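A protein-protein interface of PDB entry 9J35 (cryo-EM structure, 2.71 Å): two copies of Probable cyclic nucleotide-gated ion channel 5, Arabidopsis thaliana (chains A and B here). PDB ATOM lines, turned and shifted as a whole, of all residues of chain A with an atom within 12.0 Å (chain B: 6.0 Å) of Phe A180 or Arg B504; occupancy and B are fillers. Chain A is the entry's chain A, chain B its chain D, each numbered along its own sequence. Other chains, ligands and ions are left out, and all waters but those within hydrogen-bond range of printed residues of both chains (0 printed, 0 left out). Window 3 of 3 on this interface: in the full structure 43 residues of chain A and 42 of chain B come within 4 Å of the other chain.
Hydrophobic or aromatic side chains of chain B that line the printed part of chain A: Ala B500, Leu B501 and Ile B548.
Of the 13 printed residues of chain A, 1 touches a printed residue of chain B.
Printed residues of chain A that touch a printed residue of chain B: Phe A180.
Hydrophobic or aromatic side chains of chain A within 4 Å of the printed part of chain B: Phe A180.
Among the printed residues, no Asp or Glu carboxylate lies within 4 Å of a Lys or Arg side-chain nitrogen of the other chain.
O of Ala B500 touches CE2 of Phe A180, at 3.3 Å.
Phe A180 touches Leu B501 (CD2 to CD2, 3.7 Å).
Arg B504 touches Phe A180 (NH1 to CE1, 3.3 Å).
O of Phe A180 sits close to O of Ile B548.
No position is printed for both chains.
Phe A180 touches just these residues of chain B: Ala B500, Leu B501, Arg B504 and Ile B548.
Of chain A, only Phe A180 (3.3 Å) comes within 4 Å of Arg B504.
Printed residues of chain A within 4 Å of Ala B500: Phe A180 (3.3 Å).
Leu B501 touches just one residue of chain A: Phe A180 (3.7 Å).
No residue of chain A comes within 4 Å of Arg B503.
No residue of chain A comes within 4 Å of Val B505.
No residue of chain A comes within 4 Å of Pro B506.
Ile B548 touches one residue of chain A.
Glu B572 touches none of the printed residues of chain A.
No residue of chain A comes within 4 Å of Gly B573.
No residue of chain A comes within 4 Å of Glu B574.
Gly A181 touches none of the printed residues of chain B.
The nearest residue of chain A that does not touch Arg B504 is Arg A178 (7.6 Å).
The guanidinium group (NE) of Arg B504 is in hydrogen-bond range of the backbone carbonyl oxygen (O) of Gly B573.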
ATOM      1  N   ILE A 173      -0.718  -8.566  -6.454  1.00  0.00           N
ATOM      2  CA  ILE A 173      -1.669  -8.084  -5.455  1.00  0.00           C
ATOM      3  C   ILE A 173      -2.406  -6.868  -6.008  1.00  0.00           C
ATOM      4  O   ILE A 173      -1.786  -5.969  -6.585  1.00  0.00           O
ATOM      5  CB  ILE A 173      -0.947  -7.729  -4.136  1.00  0.00           C
ATOM      6  CG1 ILE A 173      -0.077  -8.889  -3.679  1.00  0.00           C
ATOM      7  CG2 ILE A 173      -1.919  -7.379  -3.038  1.00  0.00           C
ATOM      8  CD1 ILE A 173       0.830  -8.542  -2.535  1.00  0.00           C
ATOM      9  N   ALA A 174      -3.730  -6.835  -5.818  1.00  0.00           N
ATOM     10  CA  ALA A 174      -4.599  -5.768  -6.302  1.00  0.00           C
ATOM     11  C   ALA A 174      -5.530  -5.311  -5.181  1.00  0.00           C
ATOM     12  O   ALA A 174      -5.779  -6.085  -4.250  1.00  0.00           O
ATOM     13  CB  ALA A 174      -5.391  -6.264  -7.514  1.00  0.00           C
ATOM     14  N   PRO A 175      -6.058  -4.082  -5.209  1.00  0.00           N
ATOM     15  CA  PRO A 175      -6.935  -3.645  -4.118  1.00  0.00           C
ATOM     16  C   PRO A 175      -8.329  -4.243  -4.219  1.00  0.00           C
ATOM     17  O   PRO A 175      -8.834  -4.546  -5.303  1.00  0.00           O
ATOM     18  CB  PRO A 175      -6.978  -2.124  -4.282  1.00  0.00           C
ATOM     19  CG  PRO A 175      -6.721  -1.902  -5.690  1.00  0.00           C
ATOM     20  CD  PRO A 175      -5.742  -2.958  -6.107  1.00  0.00           C
ATOM     21  N   SER A 176      -8.952  -4.392  -3.053  1.00  0.00           N
ATOM     22  CA  SER A 176     -10.283  -4.960  -2.884  1.00  0.00           C
ATOM     23  C   SER A 176     -10.733  -4.670  -1.462  1.00  0.00           C
ATOM     24  O   SER A 176      -9.910  -4.472  -0.567  1.00  0.00           O
ATOM     25  CB  SER A 176     -10.298  -6.468  -3.162  1.00  0.00           C
ATOM     26  OG  SER A 176     -11.553  -7.035  -2.851  1.00  0.00           O
ATOM     27  N   SER A 177     -12.051  -4.632  -1.264  1.00  0.00           N
ATOM     28  CA  SER A 177     -12.614  -4.444   0.066  1.00  0.00           C
ATOM     29  C   SER A 177     -13.193  -5.717   0.667  1.00  0.00           C
ATOM     30  O   SER A 177     -13.768  -5.660   1.757  1.00  0.00           O
ATOM     31  CB  SER A 177     -13.707  -3.366   0.042  1.00  0.00           C
ATOM     32  OG  SER A 177     -14.215  -3.142   1.344  1.00  0.00           O
ATOM     33  N   ARG A 178     -13.048  -6.853  -0.009  1.00  0.00           N
ATOM     34  CA  ARG A 178     -13.483  -8.165   0.465  1.00  0.00           C
ATOM     35  C   ARG A 178     -12.308  -8.997   0.964  1.00  0.00           C
ATOM     36  O   ARG A 178     -12.239 -10.202   0.713  1.00  0.00           O
ATOM     37  CB  ARG A 178     -14.221  -8.901  -0.649  1.00  0.00           C
ATOM     38  CG  ARG A 178     -15.318  -8.088  -1.334  1.00  0.00           C
ATOM     39  CD  ARG A 178     -16.563  -7.891  -0.454  1.00  0.00           C
ATOM     40  NE  ARG A 178     -17.080  -9.139   0.114  1.00  0.00           N
ATOM     41  CZ  ARG A 178     -16.948  -9.512   1.386  1.00  0.00           C
ATOM     42  NH1 ARG A 178     -17.445 -10.670   1.793  1.00  0.00           N
ATOM     43  NH2 ARG A 178     -16.318  -8.731   2.250  1.00  0.00           N
ATOM     44  N   VAL A 179     -11.365  -8.377   1.670  1.00  0.00           N
ATOM     45  CA  VAL A 179     -10.015  -8.921   1.773  1.00  0.00           C
ATOM     46  C   VAL A 179      -9.667  -9.589   3.101  1.00  0.00           C
ATOM     47  O   VAL A 179      -9.181 -10.725   3.098  1.00  0.00           O
ATOM     48  CB  VAL A 179      -8.986  -7.824   1.434  1.00  0.00           C
ATOM     49  CG1 VAL A 179      -8.901  -7.669  -0.042  1.00  0.00           C
ATOM     50  CG2 VAL A 179      -9.398  -6.478   2.022  1.00  0.00           C
ATOM     51  N   PHE A 180      -9.857  -8.873   4.222  1.00  0.00           N
ATOM     52  CA  PHE A 180      -9.271  -9.109   5.552  1.00  0.00           C
ATOM     53  C   PHE A 180      -7.745  -9.049   5.577  1.00  0.00           C
ATOM     54  O   PHE A 180      -7.150  -9.391   6.601  1.00  0.00           O
ATOM     55  CB  PHE A 180      -9.673 -10.463   6.166  1.00  0.00           C
ATOM     56  CG  PHE A 180     -11.123 -10.601   6.484  1.00  0.00           C
ATOM     57  CD1 PHE A 180     -11.775 -11.794   6.236  1.00  0.00           C
ATOM     58  CD2 PHE A 180     -11.827  -9.560   7.059  1.00  0.00           C
ATOM     59  CE1 PHE A 180     -13.112 -11.944   6.540  1.00  0.00           C
ATOM     60  CE2 PHE A 180     -13.165  -9.702   7.362  1.00  0.00           C
ATOM     61  CZ  PHE A 180     -13.809 -10.897   7.103  1.00  0.00           C
ATOM     62  N   GLY A 181      -7.090  -8.676   4.477  1.00  0.00           N
ATOM     63  CA  GLY A 181      -5.639  -8.699   4.443  1.00  0.00           C
ATOM     64  C   GLY A 181      -4.963  -7.660   3.575  1.00  0.00           C
ATOM     65  O   GLY A 181      -3.769  -7.787   3.297  1.00  0.00           O
ATOM     66  N   ARG A 182      -5.707  -6.652   3.127  1.00  0.00           N
ATOM     67  CA  ARG A 182      -5.272  -5.516   2.304  1.00  0.00           C
ATOM     68  C   ARG A 182      -4.777  -5.939   0.931  1.00  0.00           C
ATOM     69  O   ARG A 182      -3.698  -5.508   0.531  1.00  0.00           O
ATOM     70  CB  ARG A 182      -4.187  -4.643   2.961  1.00  0.00           C
ATOM     71  CG  ARG A 182      -4.722  -3.759   4.044  1.00  0.00           C
ATOM     72  CD  ARG A 182      -4.643  -4.467   5.345  1.00  0.00           C
ATOM     73  NE  ARG A 182      -5.299  -3.716   6.390  1.00  0.00           N
ATOM     74  CZ  ARG A 182      -6.569  -3.895   6.720  1.00  0.00           C
ATOM     75  NH1 ARG A 182      -7.311  -4.793   6.086  1.00  0.00           N
ATOM     76  NH2 ARG A 182      -7.096  -3.171   7.684  1.00  0.00           N
ATOM     77  N   GLY A 183      -5.516  -6.769   0.206  1.00  0.00           N
ATOM     78  CA  GLY A 183      -5.147  -7.100  -1.150  1.00  0.00           C
ATOM     79  C   GLY A 183      -5.516  -8.497  -1.591  1.00  0.00           C
ATOM     80  O   GLY A 183      -5.191  -9.481  -0.924  1.00  0.00           O
ATOM     81  N   GLU A 184      -6.179  -8.582  -2.742  1.00  0.00           N
ATOM     82  CA  GLU A 184      -6.573  -9.843  -3.358  1.00  0.00           C
ATOM     83  C   GLU A 184      -5.422 -10.334  -4.231  1.00  0.00           C
ATOM     84  O   GLU A 184      -4.837  -9.557  -4.991  1.00  0.00           O
ATOM     85  CB  GLU A 184      -7.838  -9.637  -4.187  1.00  0.00           C
ATOM     86  CG  GLU A 184      -8.440 -10.886  -4.807  1.00  0.00           C
ATOM     87  CD  GLU A 184      -9.103 -11.790  -3.785  1.00  0.00           C
ATOM     88  OE1 GLU A 184      -9.526 -11.287  -2.723  1.00  0.00           O
ATOM     89  OE2 GLU A 184      -9.211 -13.003  -4.051  1.00  0.00           O
ATOM     90  N   LEU A 185      -5.094 -11.618  -4.123  1.00  0.00           N
ATOM     91  CA  LEU A 185      -4.069 -12.218  -4.966  1.00  0.00           C
ATOM     92  C   LEU A 185      -4.687 -12.721  -6.264  1.00  0.00           C
ATOM     93  O   LEU A 185      -5.681 -13.451  -6.248  1.00  0.00           O
ATOM     94  CB  LEU A 185      -3.391 -13.371  -4.230  1.00  0.00           C
ATOM     95  CG  LEU A 185      -1.916 -13.640  -4.496  1.00  0.00           C
ATOM     96  CD1 LEU A 185      -1.077 -12.458  -4.063  1.00  0.00           C
ATOM     97  CD2 LEU A 185      -1.477 -14.885  -3.762  1.00  0.00           C
ATOM     98  N   LEU B 499     -14.550  -2.244   8.279  1.00  0.00           N
ATOM     99  CA  LEU B 499     -15.988  -2.502   8.347  1.00  0.00           C
ATOM    100  C   LEU B 499     -16.348  -3.983   8.280  1.00  0.00           C
ATOM    101  O   LEU B 499     -17.181  -4.457   9.066  1.00  0.00           O
ATOM    102  CB  LEU B 499     -16.714  -1.755   7.233  1.00  0.00           C
ATOM    103  CG  LEU B 499     -18.219  -1.583   7.432  1.00  0.00           C
ATOM    104  CD1 LEU B 499     -18.513  -0.593   8.542  1.00  0.00           C
ATOM    105  CD2 LEU B 499     -18.868  -1.143   6.142  1.00  0.00           C
ATOM    106  N   ALA B 500     -15.715  -4.734   7.380  1.00  0.00           N
ATOM    107  CA  ALA B 500     -15.937  -6.169   7.288  1.00  0.00           C
ATOM    108  C   ALA B 500     -15.370  -6.935   8.475  1.00  0.00           C
ATOM    109  O   ALA B 500     -15.714  -8.103   8.652  1.00  0.00           O
ATOM    110  CB  ALA B 500     -15.330  -6.707   5.996  1.00  0.00           C
ATOM    111  N   LEU B 501     -14.505  -6.323   9.282  1.00  0.00           N
ATOM    112  CA  LEU B 501     -14.046  -6.971  10.505  1.00  0.00           C
ATOM    113  C   LEU B 501     -15.067  -6.825  11.620  1.00  0.00           C
ATOM    114  O   LEU B 501     -15.368  -7.792  12.320  1.00  0.00           O
ATOM    115  CB  LEU B 501     -12.706  -6.390  10.953  1.00  0.00           C
ATOM    116  CG  LEU B 501     -11.466  -6.771  10.162  1.00  0.00           C
ATOM    117  CD1 LEU B 501     -10.335  -5.847  10.530  1.00  0.00           C
ATOM    118  CD2 LEU B 501     -11.096  -8.209  10.439  1.00  0.00           C
ATOM    119  N   VAL B 502     -15.607  -5.620  11.809  1.00  0.00           N
ATOM    120  CA  VAL B 502     -16.574  -5.418  12.878  1.00  0.00           C
ATOM    121  C   VAL B 502     -17.950  -5.940  12.498  1.00  0.00           C
ATOM    122  O   VAL B 502     -18.820  -6.061  13.364  1.00  0.00           O
ATOM    123  CB  VAL B 502     -16.657  -3.938  13.285  1.00  0.00           C
ATOM    124  CG1 VAL B 502     -15.277  -3.379  13.522  1.00  0.00           C
ATOM    125  CG2 VAL B 502     -17.384  -3.146  12.232  1.00  0.00           C
ATOM    126  N   ARG B 503     -18.184  -6.265  11.229  1.00  0.00           N
ATOM    127  CA  ARG B 503     -19.412  -6.976  10.878  1.00  0.00           C
ATOM    128  C   ARG B 503     -19.223  -8.491  10.950  1.00  0.00           C
ATOM    129  O   ARG B 503     -19.605  -9.242  10.055  1.00  0.00           O
ATOM    130  CB  ARG B 503     -19.874  -6.563   9.491  1.00  0.00           C
ATOM    131  CG  ARG B 503     -20.742  -5.335   9.430  1.00  0.00           C
ATOM    132  CD  ARG B 503     -21.468  -5.273   8.091  1.00  0.00           C
ATOM    133  NE  ARG B 503     -20.571  -4.978   6.977  1.00  0.00           N
ATOM    134  CZ  ARG B 503     -20.097  -5.880   6.117  1.00  0.00           C
ATOM    135  NH1 ARG B 503     -20.421  -7.159   6.236  1.00  0.00           N
ATOM    136  NH2 ARG B 503     -19.283  -5.501   5.142  1.00  0.00           N
ATOM    137  N   ARG B 504     -18.629  -8.943  12.044  1.00  0.00           N
ATOM    138  CA  ARG B 504     -18.549 -10.351  12.377  1.00  0.00           C
ATOM    139  C   ARG B 504     -18.791 -10.584  13.856  1.00  0.00           C
ATOM    140  O   ARG B 504     -18.908 -11.739  14.271  1.00  0.00           O
ATOM    141  CB  ARG B 504     -17.194 -10.929  11.963  1.00  0.00           C
ATOM    142  CG  ARG B 504     -17.182 -11.442  10.542  1.00  0.00           C
ATOM    143  CD  ARG B 504     -15.784 -11.712  10.061  1.00  0.00           C
ATOM    144  NE  ARG B 504     -15.311 -13.034  10.454  1.00  0.00           N
ATOM    145  CZ  ARG B 504     -15.034 -14.009   9.595  1.00  0.00           C
ATOM    146  NH1 ARG B 504     -15.193 -13.806   8.296  1.00  0.00           N
ATOM    147  NH2 ARG B 504     -14.600 -15.183  10.030  1.00  0.00           N
ATOM    148  N   VAL B 505     -18.853  -9.530  14.659  1.00  0.00           N
ATOM    149  CA  VAL B 505     -19.326  -9.611  16.031  1.00  0.00           C
ATOM    150  C   VAL B 505     -20.845  -9.585  15.957  1.00  0.00           C
ATOM    151  O   VAL B 505     -21.407  -8.689  15.309  1.00  0.00           O
ATOM    152  CB  VAL B 505     -18.783  -8.456  16.880  1.00  0.00           C
ATOM    153  CG1 VAL B 505     -19.378  -8.489  18.263  1.00  0.00           C
ATOM    154  CG2 VAL B 505     -17.272  -8.512  16.941  1.00  0.00           C
ATOM    155  N   PRO B 506     -21.548 -10.546  16.567  1.00  0.00           N
ATOM    156  CA  PRO B 506     -23.011 -10.581  16.426  1.00  0.00           C
ATOM    157  C   PRO B 506     -23.723  -9.467  17.170  1.00  0.00           C
ATOM    158  O   PRO B 506     -24.811  -9.059  16.751  1.00  0.00           O
ATOM    159  CB  PRO B 506     -23.379 -11.959  16.991  1.00  0.00           C
ATOM    160  CG  PRO B 506     -22.113 -12.741  16.947  1.00  0.00           C
ATOM    161  CD  PRO B 506     -21.039 -11.758  17.225  1.00  0.00           C
ATOM    162  N   LYS B 509     -23.575  -6.298  14.632  1.00  0.00           N
ATOM    163  CA  LYS B 509     -24.450  -6.265  13.464  1.00  0.00           C
ATOM    164  C   LYS B 509     -25.874  -5.841  13.798  1.00  0.00           C
ATOM    165  O   LYS B 509     -26.659  -5.600  12.876  1.00  0.00           O
ATOM    166  CB  LYS B 509     -24.485  -7.623  12.775  1.00  0.00           C
ATOM    167  CG  LYS B 509     -23.307  -7.890  11.879  1.00  0.00           C
ATOM    168  CD  LYS B 509     -23.486  -9.196  11.117  1.00  0.00           C
ATOM    169  CE  LYS B 509     -24.551  -9.063  10.040  1.00  0.00           C
ATOM    170  NZ  LYS B 509     -24.588 -10.240   9.135  1.00  0.00           N
ATOM    171  N   ILE B 547      -8.307  -9.976  14.209  1.00  0.00           N
ATOM    172  CA  ILE B 547      -7.133 -10.511  13.524  1.00  0.00           C
ATOM    173  C   ILE B 547      -7.202 -10.198  12.036  1.00  0.00           C
ATOM    174  O   ILE B 547      -8.198 -10.491  11.372  1.00  0.00           O
ATOM    175  CB  ILE B 547      -7.003 -12.020  13.771  1.00  0.00           C
ATOM    176  CG1 ILE B 547      -7.108 -12.328  15.261  1.00  0.00           C
ATOM    177  CG2 ILE B 547      -5.691 -12.543  13.250  1.00  0.00           C
ATOM    178  CD1 ILE B 547      -6.013 -11.731  16.096  1.00  0.00           C
ATOM    179  N   ILE B 548      -6.139  -9.596  11.513  1.00  0.00           N
ATOM    180  CA  ILE B 548      -5.991  -9.320  10.084  1.00  0.00           C
ATOM    181  C   ILE B 548      -5.192 -10.416   9.396  1.00  0.00           C
ATOM    182  O   ILE B 548      -5.589 -10.929   8.354  1.00  0.00           O
ATOM    183  CB  ILE B 548      -5.315  -7.945   9.881  1.00  0.00           C
ATOM    184  CG1 ILE B 548      -6.211  -6.807  10.311  1.00  0.00           C
ATOM    185  CG2 ILE B 548      -4.886  -7.728   8.457  1.00  0.00           C
ATOM    186  CD1 ILE B 548      -5.442  -5.562  10.462  1.00  0.00           C
ATOM    187  N   ARG B 549      -4.061 -10.785   9.979  1.00  0.00           N
ATOM    188  CA  ARG B 549      -3.122 -11.725   9.403  1.00  0.00           C
ATOM    189  C   ARG B 549      -2.603 -12.604  10.525  1.00  0.00           C
ATOM    190  O   ARG B 549      -2.675 -12.231  11.694  1.00  0.00           O
ATOM    191  CB  ARG B 549      -1.974 -10.983   8.715  1.00  0.00           C
ATOM    192  CG  ARG B 549      -1.214 -11.752   7.660  1.00  0.00           C
ATOM    193  CD  ARG B 549       0.092 -11.045   7.299  1.00  0.00           C
ATOM    194  NE  ARG B 549       0.988 -10.930   8.454  1.00  0.00           N
ATOM    195  CZ  ARG B 549       2.195 -10.364   8.429  1.00  0.00           C
ATOM    196  NH1 ARG B 549       2.678  -9.846   7.312  1.00  0.00           N
ATOM    197  NH2 ARG B 549       2.920 -10.304   9.533  1.00  0.00           N
ATOM    198  N   LYS B 571      -7.902 -17.822  13.418  1.00  0.00           N
ATOM    199  CA  LYS B 571      -7.254 -17.378  12.192  1.00  0.00           C
ATOM    200  C   LYS B 571      -7.853 -16.033  11.791  1.00  0.00           C
ATOM    201  O   LYS B 571      -8.524 -15.379  12.594  1.00  0.00           O
ATOM    202  CB  LYS B 571      -7.364 -18.454  11.097  1.00  0.00           C
ATOM    203  CG  LYS B 571      -8.764 -18.713  10.571  1.00  0.00           C
ATOM    204  CD  LYS B 571      -8.742 -19.701   9.429  1.00  0.00           C
ATOM    205  CE  LYS B 571     -10.139 -19.919   8.879  1.00  0.00           C
ATOM    206  NZ  LYS B 571     -10.674 -18.686   8.237  1.00  0.00           N
ATOM    207  N   GLU B 572      -7.595 -15.625  10.548  1.00  0.00           N
ATOM    208  CA  GLU B 572      -7.892 -14.283  10.067  1.00  0.00           C
ATOM    209  C   GLU B 572      -9.392 -14.036  10.003  1.00  0.00           C
ATOM    210  O   GLU B 572     -10.144 -14.842   9.450  1.00  0.00           O
ATOM    211  CB  GLU B 572      -7.289 -14.105   8.682  1.00  0.00           C
ATOM    212  CG  GLU B 572      -5.841 -14.481   8.634  1.00  0.00           C
ATOM    213  CD  GLU B 572      -5.234 -14.312   7.266  1.00  0.00           C
ATOM    214  OE1 GLU B 572      -5.961 -13.899   6.343  1.00  0.00           O
ATOM    215  OE2 GLU B 572      -4.035 -14.621   7.109  1.00  0.00           O
ATOM    216  N   GLY B 573      -9.825 -12.915  10.553  1.00  0.00           N
ATOM    217  CA  GLY B 573     -11.220 -12.558  10.603  1.00  0.00           C
ATOM    218  C   GLY B 573     -11.850 -12.760  11.957  1.00  0.00           C
ATOM    219  O   GLY B 573     -12.870 -12.131  12.249  1.00  0.00           O
ATOM    220  N   GLU B 574     -11.271 -13.604  12.793  1.00  0.00           N
ATOM    221  CA  GLU B 574     -11.845 -13.895  14.095  1.00  0.00           C
ATOM    222  C   GLU B 574     -11.359 -12.878  15.117  1.00  0.00           C
ATOM    223  O   GLU B 574     -10.451 -12.093  14.857  1.00  0.00           O
ATOM    224  CB  GLU B 574     -11.491 -15.319  14.517  1.00  0.00           C
ATOM    225  CG  GLU B 574     -11.764 -16.342  13.419  1.00  0.00           C
ATOM    226  CD  GLU B 574     -11.443 -17.767  13.827  1.00  0.00           C
ATOM    227  OE1 GLU B 574     -11.660 -18.118  15.002  1.00  0.00           O
ATOM    228  OE2 GLU B 574     -10.979 -18.541  12.971  1.00  0.00           O
ATOM    229  N   PHE B 575     -11.982 -12.883  16.283  1.00  0.00           N
ATOM    230  CA  PHE B 575     -11.684 -11.873  17.282  1.00  0.00           C
ATOM    231  C   PHE B 575     -11.393 -12.524  18.630  1.00  0.00           C
ATOM    232  O   PHE B 575     -11.330 -13.743  18.752  1.00  0.00           O
ATOM    233  CB  PHE B 575     -12.810 -10.833  17.369  1.00  0.00           C
ATOM    234  CG  PHE B 575     -14.109 -11.359  17.897  1.00  0.00           C
ATOM    235  CD1 PHE B 575     -14.485 -11.106  19.201  1.00  0.00           C
ATOM    236  CD2 PHE B 575     -14.980 -12.057  17.076  1.00  0.00           C
ATOM    237  CE1 PHE B 575     -15.679 -11.572  19.688  1.00  0.00           C
ATOM    238  CE2 PHE B 575     -16.173 -12.525  17.560  1.00  0.00           C
ATOM    239  CZ  PHE B 575     -16.524 -12.281  18.871  1.00  0.00           C
